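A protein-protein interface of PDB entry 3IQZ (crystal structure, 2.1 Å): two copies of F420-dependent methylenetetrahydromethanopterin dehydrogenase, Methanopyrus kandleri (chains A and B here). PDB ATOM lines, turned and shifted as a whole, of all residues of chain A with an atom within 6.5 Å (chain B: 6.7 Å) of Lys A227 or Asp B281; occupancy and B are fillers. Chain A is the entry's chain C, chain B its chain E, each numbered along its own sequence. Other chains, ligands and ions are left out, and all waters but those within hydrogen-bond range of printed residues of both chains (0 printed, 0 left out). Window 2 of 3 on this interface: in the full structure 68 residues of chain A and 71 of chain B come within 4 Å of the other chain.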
ATOM      1  N   GLU A 130     -11.322  31.134   4.968  1.00  0.00           N
ATOM      2  CA  GLU A 130      -9.898  30.788   4.965  1.00  0.00           C
ATOM      3  C   GLU A 130      -9.328  30.760   3.572  1.00  0.00           C
ATOM      4  O   GLU A 130      -8.109  30.666   3.430  1.00  0.00           O
ATOM      5  CB  GLU A 130      -9.629  29.432   5.597  1.00  0.00           C
ATOM      6  CG  GLU A 130     -10.146  29.294   7.036  1.00  0.00           C
ATOM      7  CD  GLU A 130     -11.573  28.793   7.055  1.00  0.00           C
ATOM      8  OE1 GLU A 130     -11.983  28.209   8.067  1.00  0.00           O
ATOM      9  OE2 GLU A 130     -12.267  28.941   6.030  1.00  0.00           O
ATOM     10  N   GLU A 224     -18.666  19.304   4.528  1.00  0.00           N
ATOM     11  CA  GLU A 224     -17.439  19.083   5.291  1.00  0.00           C
ATOM     12  C   GLU A 224     -17.265  20.169   6.370  1.00  0.00           C
ATOM     13  O   GLU A 224     -17.239  21.328   6.063  1.00  0.00           O
ATOM     14  CB  GLU A 224     -16.216  19.045   4.349  1.00  0.00           C
ATOM     15  CG  GLU A 224     -14.893  18.822   5.071  1.00  0.00           C
ATOM     16  CD  GLU A 224     -14.832  17.484   5.781  1.00  0.00           C
ATOM     17  OE1 GLU A 224     -14.779  17.496   7.016  1.00  0.00           O
ATOM     18  OE2 GLU A 224     -14.824  16.411   5.128  1.00  0.00           O
ATOM     19  N   GLN A 225     -17.115  19.763   7.626  1.00  0.00           N
ATOM     20  CA  GLN A 225     -16.976  20.698   8.751  1.00  0.00           C
ATOM     21  C   GLN A 225     -15.543  20.884   9.273  1.00  0.00           C
ATOM     22  O   GLN A 225     -15.290  21.852   9.987  1.00  0.00           O
ATOM     23  CB  GLN A 225     -17.878  20.259   9.909  1.00  0.00           C
ATOM     24  CG  GLN A 225     -19.296  20.050   9.469  1.00  0.00           C
ATOM     25  CD  GLN A 225     -19.935  21.363   9.036  1.00  0.00           C
ATOM     26  OE1 GLN A 225     -20.128  22.248   9.860  1.00  0.00           O
ATOM     27  NE2 GLN A 225     -20.255  21.502   7.750  1.00  0.00           N
ATOM     28  N   ASP A 226     -14.639  19.945   8.950  1.00  0.00           N
ATOM     29  CA  ASP A 226     -13.225  20.015   9.348  1.00  0.00           C
ATOM     30  C   ASP A 226     -12.413  20.871   8.361  1.00  0.00           C
ATOM     31  O   ASP A 226     -12.222  20.461   7.208  1.00  0.00           O
ATOM     32  CB  ASP A 226     -12.672  18.573   9.389  1.00  0.00           C
ATOM     33  CG  ASP A 226     -11.212  18.497   9.779  1.00  0.00           C
ATOM     34  OD1 ASP A 226     -10.723  17.343  10.012  1.00  0.00           O
ATOM     35  OD2 ASP A 226     -10.557  19.563   9.856  1.00  0.00           O
ATOM     36  N   LYS A 227     -11.942  22.046   8.802  1.00  0.00           N
ATOM     37  CA  LYS A 227     -11.224  22.992   7.916  1.00  0.00           C
ATOM     38  C   LYS A 227      -9.914  22.412   7.314  1.00  0.00           C
ATOM     39  O   LYS A 227      -9.389  22.904   6.324  1.00  0.00           O
ATOM     40  CB  LYS A 227     -10.920  24.305   8.642  1.00  0.00           C
ATOM     41  CG  LYS A 227      -9.939  24.148   9.741  1.00  0.00           C
ATOM     42  CD  LYS A 227      -9.501  25.458  10.358  1.00  0.00           C
ATOM     43  CE  LYS A 227      -8.511  25.187  11.508  1.00  0.00           C
ATOM     44  NZ  LYS A 227      -7.791  26.418  11.906  1.00  0.00           N
ATOM     45  N   GLU A 228      -9.372  21.378   7.925  1.00  0.00           N
ATOM     46  CA  GLU A 228      -8.213  20.722   7.323  1.00  0.00           C
ATOM     47  C   GLU A 228      -8.623  19.979   6.069  1.00  0.00           C
ATOM     48  O   GLU A 228      -7.794  19.654   5.222  1.00  0.00           O
ATOM     49  CB  GLU A 228      -7.523  19.775   8.316  1.00  0.00           C
ATOM     50  CG  GLU A 228      -6.213  20.347   8.829  1.00  0.00           C
ATOM     51  CD  GLU A 228      -5.854  19.849  10.199  1.00  0.00           C
ATOM     52  OE1 GLU A 228      -5.344  20.667  10.994  1.00  0.00           O
ATOM     53  OE2 GLU A 228      -6.074  18.643  10.486  1.00  0.00           O
ATOM     54  N   ARG A 229      -9.929  19.743   5.948  1.00  0.00           N
ATOM     55  CA  ARG A 229     -10.486  19.091   4.767  1.00  0.00           C
ATOM     56  C   ARG A 229     -11.136  20.100   3.865  1.00  0.00           C
ATOM     57  O   ARG A 229     -10.931  20.080   2.648  1.00  0.00           O
ATOM     58  CB  ARG A 229     -11.454  17.951   5.148  1.00  0.00           C
ATOM     59  CG  ARG A 229     -10.772  16.795   5.918  1.00  0.00           C
ATOM     60  CD  ARG A 229     -11.764  15.751   6.432  1.00  0.00           C
ATOM     61  NE  ARG A 229     -12.498  15.099   5.354  1.00  0.00           N
ATOM     62  CZ  ARG A 229     -12.070  14.027   4.682  1.00  0.00           C
ATOM     63  NH1 ARG A 229     -12.822  13.520   3.712  1.00  0.00           N
ATOM     64  NH2 ARG A 229     -10.905  13.442   4.965  1.00  0.00           N
ATOM     65  N   TYR A 230     -11.927  21.000   4.438  1.00  0.00           N
ATOM     66  CA  TYR A 230     -12.706  21.867   3.585  1.00  0.00           C
ATOM     67  C   TYR A 230     -11.943  22.971   2.840  1.00  0.00           C
ATOM     68  O   TYR A 230     -12.375  23.383   1.757  1.00  0.00           O
ATOM     69  CB  TYR A 230     -13.990  22.382   4.267  1.00  0.00           C
ATOM     70  CG  TYR A 230     -13.867  23.424   5.357  1.00  0.00           C
ATOM     71  CD1 TYR A 230     -14.383  23.173   6.651  1.00  0.00           C
ATOM     72  CD2 TYR A 230     -13.305  24.669   5.107  1.00  0.00           C
ATOM     73  CE1 TYR A 230     -14.337  24.150   7.669  1.00  0.00           C
ATOM     74  CE2 TYR A 230     -13.245  25.641   6.126  1.00  0.00           C
ATOM     75  CZ  TYR A 230     -13.745  25.368   7.391  1.00  0.00           C
ATOM     76  OH  TYR A 230     -13.692  26.374   8.331  1.00  0.00           O
ATOM     77  N   VAL A 231     -10.845  23.465   3.400  1.00  0.00           N
ATOM     78  CA  VAL A 231     -10.047  24.444   2.672  1.00  0.00           C
ATOM     79  C   VAL A 231      -9.464  23.824   1.368  1.00  0.00           C
ATOM     80  O   VAL A 231      -9.698  24.352   0.271  1.00  0.00           O
ATOM     81  CB  VAL A 231      -8.977  25.097   3.557  1.00  0.00           C
ATOM     82  CG1 VAL A 231      -8.239  26.195   2.793  1.00  0.00           C
ATOM     83  CG2 VAL A 231      -9.614  25.676   4.831  1.00  0.00           C
ATOM     84  N   PRO A 232      -8.769  22.674   1.463  1.00  0.00           N
ATOM     85  CA  PRO A 232      -8.295  22.053   0.226  1.00  0.00           C
ATOM     86  C   PRO A 232      -9.418  21.734  -0.722  1.00  0.00           C
ATOM     87  O   PRO A 232      -9.258  21.867  -1.928  1.00  0.00           O
ATOM     88  CB  PRO A 232      -7.660  20.730   0.705  1.00  0.00           C
ATOM     89  CG  PRO A 232      -7.264  20.983   2.095  1.00  0.00           C
ATOM     90  CD  PRO A 232      -8.242  21.996   2.672  1.00  0.00           C
ATOM     91  N   SER B 274      -5.720  38.622   7.294  1.00  0.00           N
ATOM     92  CA  SER B 274      -4.619  38.419   6.403  1.00  0.00           C
ATOM     93  C   SER B 274      -3.980  37.057   6.579  1.00  0.00           C
ATOM     94  O   SER B 274      -3.946  36.500   7.676  1.00  0.00           O
ATOM     95  CB  SER B 274      -3.574  39.509   6.605  1.00  0.00           C
ATOM     96  OG  SER B 274      -2.466  39.241   5.760  1.00  0.00           O
ATOM     97  N   LYS B 275      -3.458  36.510   5.493  1.00  0.00           N
ATOM     98  CA  LYS B 275      -2.627  35.291   5.609  1.00  0.00           C
ATOM     99  C   LYS B 275      -1.850  35.110   4.318  1.00  0.00           C
ATOM    100  O   LYS B 275      -2.122  35.819   3.305  1.00  0.00           O
ATOM    101  CB  LYS B 275      -3.508  34.055   5.810  1.00  0.00           C
ATOM    102  CG  LYS B 275      -4.653  33.973   4.724  1.00  0.00           C
ATOM    103  CD  LYS B 275      -5.447  32.665   4.825  1.00  0.00           C
ATOM    104  CE  LYS B 275      -4.699  31.451   4.264  1.00  0.00           C
ATOM    105  NZ  LYS B 275      -5.547  30.258   4.482  1.00  0.00           N
ATOM    106  N   ARG B 276      -0.962  34.114   4.339  1.00  0.00           N
ATOM    107  CA  ARG B 276      -0.101  33.725   3.220  1.00  0.00           C
ATOM    108  C   ARG B 276      -0.036  32.192   3.043  1.00  0.00           C
ATOM    109  O   ARG B 276      -0.061  31.681   1.940  1.00  0.00           O
ATOM    110  CB  ARG B 276       1.339  34.190   3.461  1.00  0.00           C
ATOM    111  CG  ARG B 276       1.528  35.701   3.405  1.00  0.00           C
ATOM    112  CD  ARG B 276       2.037  36.078   2.043  1.00  0.00           C
ATOM    113  NE  ARG B 276       2.180  37.507   1.861  1.00  0.00           N
ATOM    114  CZ  ARG B 276       2.353  38.047   0.669  1.00  0.00           C
ATOM    115  NH1 ARG B 276       2.461  39.365   0.520  1.00  0.00           N
ATOM    116  NH2 ARG B 276       2.414  37.230  -0.379  1.00  0.00           N
ATOM    117  N   LYS B 277       0.096  31.460   4.133  1.00  0.00           N
ATOM    118  CA  LYS B 277       0.128  30.000   4.031  1.00  0.00           C
ATOM    119  C   LYS B 277      -1.254  29.395   3.821  1.00  0.00           C
ATOM    120  O   LYS B 277      -2.211  29.786   4.468  1.00  0.00           O
ATOM    121  CB  LYS B 277       0.827  29.398   5.249  1.00  0.00           C
ATOM    122  CG  LYS B 277       2.338  29.411   5.091  1.00  0.00           C
ATOM    123  CD  LYS B 277       2.977  29.493   6.436  1.00  0.00           C
ATOM    124  CE  LYS B 277       4.482  29.719   6.352  1.00  0.00           C
ATOM    125  NZ  LYS B 277       5.264  28.513   5.958  1.00  0.00           N
ATOM    126  N   PHE B 278      -1.362  28.457   2.897  1.00  0.00           N
ATOM    127  CA  PHE B 278      -2.666  27.891   2.526  1.00  0.00           C
ATOM    128  C   PHE B 278      -3.477  27.409   3.737  1.00  0.00           C
ATOM    129  O   PHE B 278      -4.675  27.654   3.841  1.00  0.00           O
ATOM    130  CB  PHE B 278      -2.485  26.731   1.503  1.00  0.00           C
ATOM    131  CG  PHE B 278      -3.809  26.152   0.976  1.00  0.00           C
ATOM    132  CD1 PHE B 278      -4.224  24.862   1.374  1.00  0.00           C
ATOM    133  CD2 PHE B 278      -4.622  26.880   0.148  1.00  0.00           C
ATOM    134  CE1 PHE B 278      -5.423  24.325   0.920  1.00  0.00           C
ATOM    135  CE2 PHE B 278      -5.820  26.344  -0.322  1.00  0.00           C
ATOM    136  CZ  PHE B 278      -6.215  25.061   0.064  1.00  0.00           C
ATOM    137  N   MET B 279      -2.818  26.710   4.636  1.00  0.00           N
ATOM    138  CA  MET B 279      -3.465  26.140   5.825  1.00  0.00           C
ATOM    139  C   MET B 279      -3.562  27.094   7.004  1.00  0.00           C
ATOM    140  O   MET B 279      -4.142  26.740   8.011  1.00  0.00           O
ATOM    141  CB  MET B 279      -2.729  24.879   6.315  1.00  0.00           C
ATOM    142  CG  MET B 279      -2.871  23.602   5.436  1.00  0.00           C
ATOM    143  SD  MET B 279      -4.511  23.250   4.740  1.00  0.00           S
ATOM    144  CE  MET B 279      -5.681  24.013   5.928  1.00  0.00           C
ATOM    145  N   GLU B 280      -2.964  28.270   6.906  1.00  0.00           N
ATOM    146  CA  GLU B 280      -2.943  29.167   8.034  1.00  0.00           C
ATOM    147  C   GLU B 280      -4.298  29.905   8.110  1.00  0.00           C
ATOM    148  O   GLU B 280      -4.790  30.352   7.084  1.00  0.00           O
ATOM    149  CB  GLU B 280      -1.753  30.112   7.877  1.00  0.00           C
ATOM    150  CG  GLU B 280      -2.037  31.568   8.184  1.00  0.00           C
ATOM    151  CD  GLU B 280      -0.884  32.495   7.798  1.00  0.00           C
ATOM    152  OE1 GLU B 280      -0.265  32.304   6.727  1.00  0.00           O
ATOM    153  OE2 GLU B 280      -0.600  33.428   8.583  1.00  0.00           O
ATOM    154  N   ASP B 281      -4.921  29.953   9.287  1.00  0.00           N
ATOM    155  CA  ASP B 281      -6.114  30.812   9.486  1.00  0.00           C
ATOM    156  C   ASP B 281      -5.764  32.260   9.203  1.00  0.00           C
ATOM    157  O   ASP B 281      -4.678  32.722   9.574  1.00  0.00           O
ATOM    158  CB  ASP B 281      -6.659  30.745  10.919  1.00  0.00           C
ATOM    159  CG  ASP B 281      -7.301  29.407  11.253  1.00  0.00           C
ATOM    160  OD1 ASP B 281      -7.582  28.607  10.335  1.00  0.00           O
ATOM    161  OD2 ASP B 281      -7.532  29.157  12.451  1.00  0.00           O
ATOM    162  N   PRO B 282      -6.695  32.998   8.560  1.00  0.00           N
ATOM    163  CA  PRO B 282      -6.470  34.422   8.359  1.00  0.00           C
ATOM    164  C   PRO B 282      -6.667  35.165   9.682  1.00  0.00           C
ATOM    165  O   PRO B 282      -7.527  34.783  10.475  1.00  0.00           O
ATOM    166  CB  PRO B 282      -7.528  34.815   7.296  1.00  0.00           C
ATOM    167  CG  PRO B 282      -8.627  33.826   7.448  1.00  0.00           C
ATOM    168  CD  PRO B 282      -7.976  32.535   7.995  1.00  0.00           C
ATOM    169  N   GLU B 283      -5.874  36.209   9.913  1.00  0.00           N
ATOM    170  CA  GLU B 283      -5.955  36.964  11.161  1.00  0.00           C
ATOM    171  C   GLU B 283      -5.567  38.411  11.043  1.00  0.00           C
ATOM    172  O   GLU B 283      -5.798  39.164  11.983  1.00  0.00           O
ATOM    173  CB  GLU B 283      -5.054  36.325  12.202  1.00  0.00           C
ATOM    174  CG  GLU B 283      -5.784  35.410  13.125  1.00  0.00           C
ATOM    175  CD  GLU B 283      -4.844  34.478  13.786  1.00  0.00           C
ATOM    176  OE1 GLU B 283      -5.216  33.300  13.968  1.00  0.00           O
ATOM    177  OE2 GLU B 283      -3.717  34.928  14.088  1.00  0.00           O
ATOM    178  OXT GLU B 283      -5.012  38.861  10.052  1.00  0.00           O
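Of the 10 printed residues of chain B, 5 touch a printed residue of chain A.
Printed residues of chain B that touch a printed residue of chain A: Lys B275, Phe B278, Met B279, Asp B281 and Pro B282.
Hydrophobic or aromatic side chains of chain B that line the printed part of chain A: Phe B278, Met B279 and Pro B282.
Of the 10 printed residues of chain A, 4 touch a printed residue of chain B.
Printed residues of chain A that touch a printed residue of chain B: Glu A130, Lys A227, Val A231 and Pro A232.
Hydrophobic or aromatic side chains of chain A that line the printed part of chain B: Val A231 and Pro A232.
No position is printed for both chains.
Of the 6 pairs that touch across the chains among the printed residues, none has its exchanged pair printed and touching as well.
The side-chain carboxylate of Glu A130 lies within hydrogen-bond range of the side-chain hydroxyl of Tyr A230, at 2.5 Å.
O of Lys B277 sits close to NZ of Lys B275 (3.4 Å).
The side-chain amino group of Lys B275 lies within hydrogen-bond range of the backbone carbonyl oxygen of Phe B278 (2.8 Å).
The side-chain amino group (NZ) of Lys B275 lies within hydrogen-bond range of the backbone carbonyl oxygen (O) of Glu B280, at 2.7 Å.
Lys A227 touches two residues of chain B.
Asp B281 touches just one residue of chain A: Lys A227.
Of the printed residues of chain B, Val A231 touches Phe B278.
Of the printed residues of chain A, Phe B278 touches Val A231 and Pro A232.
Of the printed residues of chain B, Pro A232 touches Phe B278 (3.7 Å).
Printed residues of chain A within 4 Å of Pro B282: Glu A130 (3.99 Å).
The nearest printed residue of chain A that does not touch Phe B278 is Glu A130 (4.6 Å).
Among the printed residues, merely in contact across the chains: Val A231 with Phe B278 (3.6 Å), Pro A232 with Phe B278 (3.7 Å), Lys A227 with Met B279 (3.9 Å) and Glu A130 with Pro B282 (3.99 Å).
The side-chain carboxylate (OD1) of Asp B281 is in salt-bridge range of the side-chain amino group (NZ) of Lys A227 (2.7 Å).
The backbone carbonyl oxygen (O) of Glu A130 is in hydrogen-bond range of the side-chain amino group (NZ) of Lys B275 (2.8 Å).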
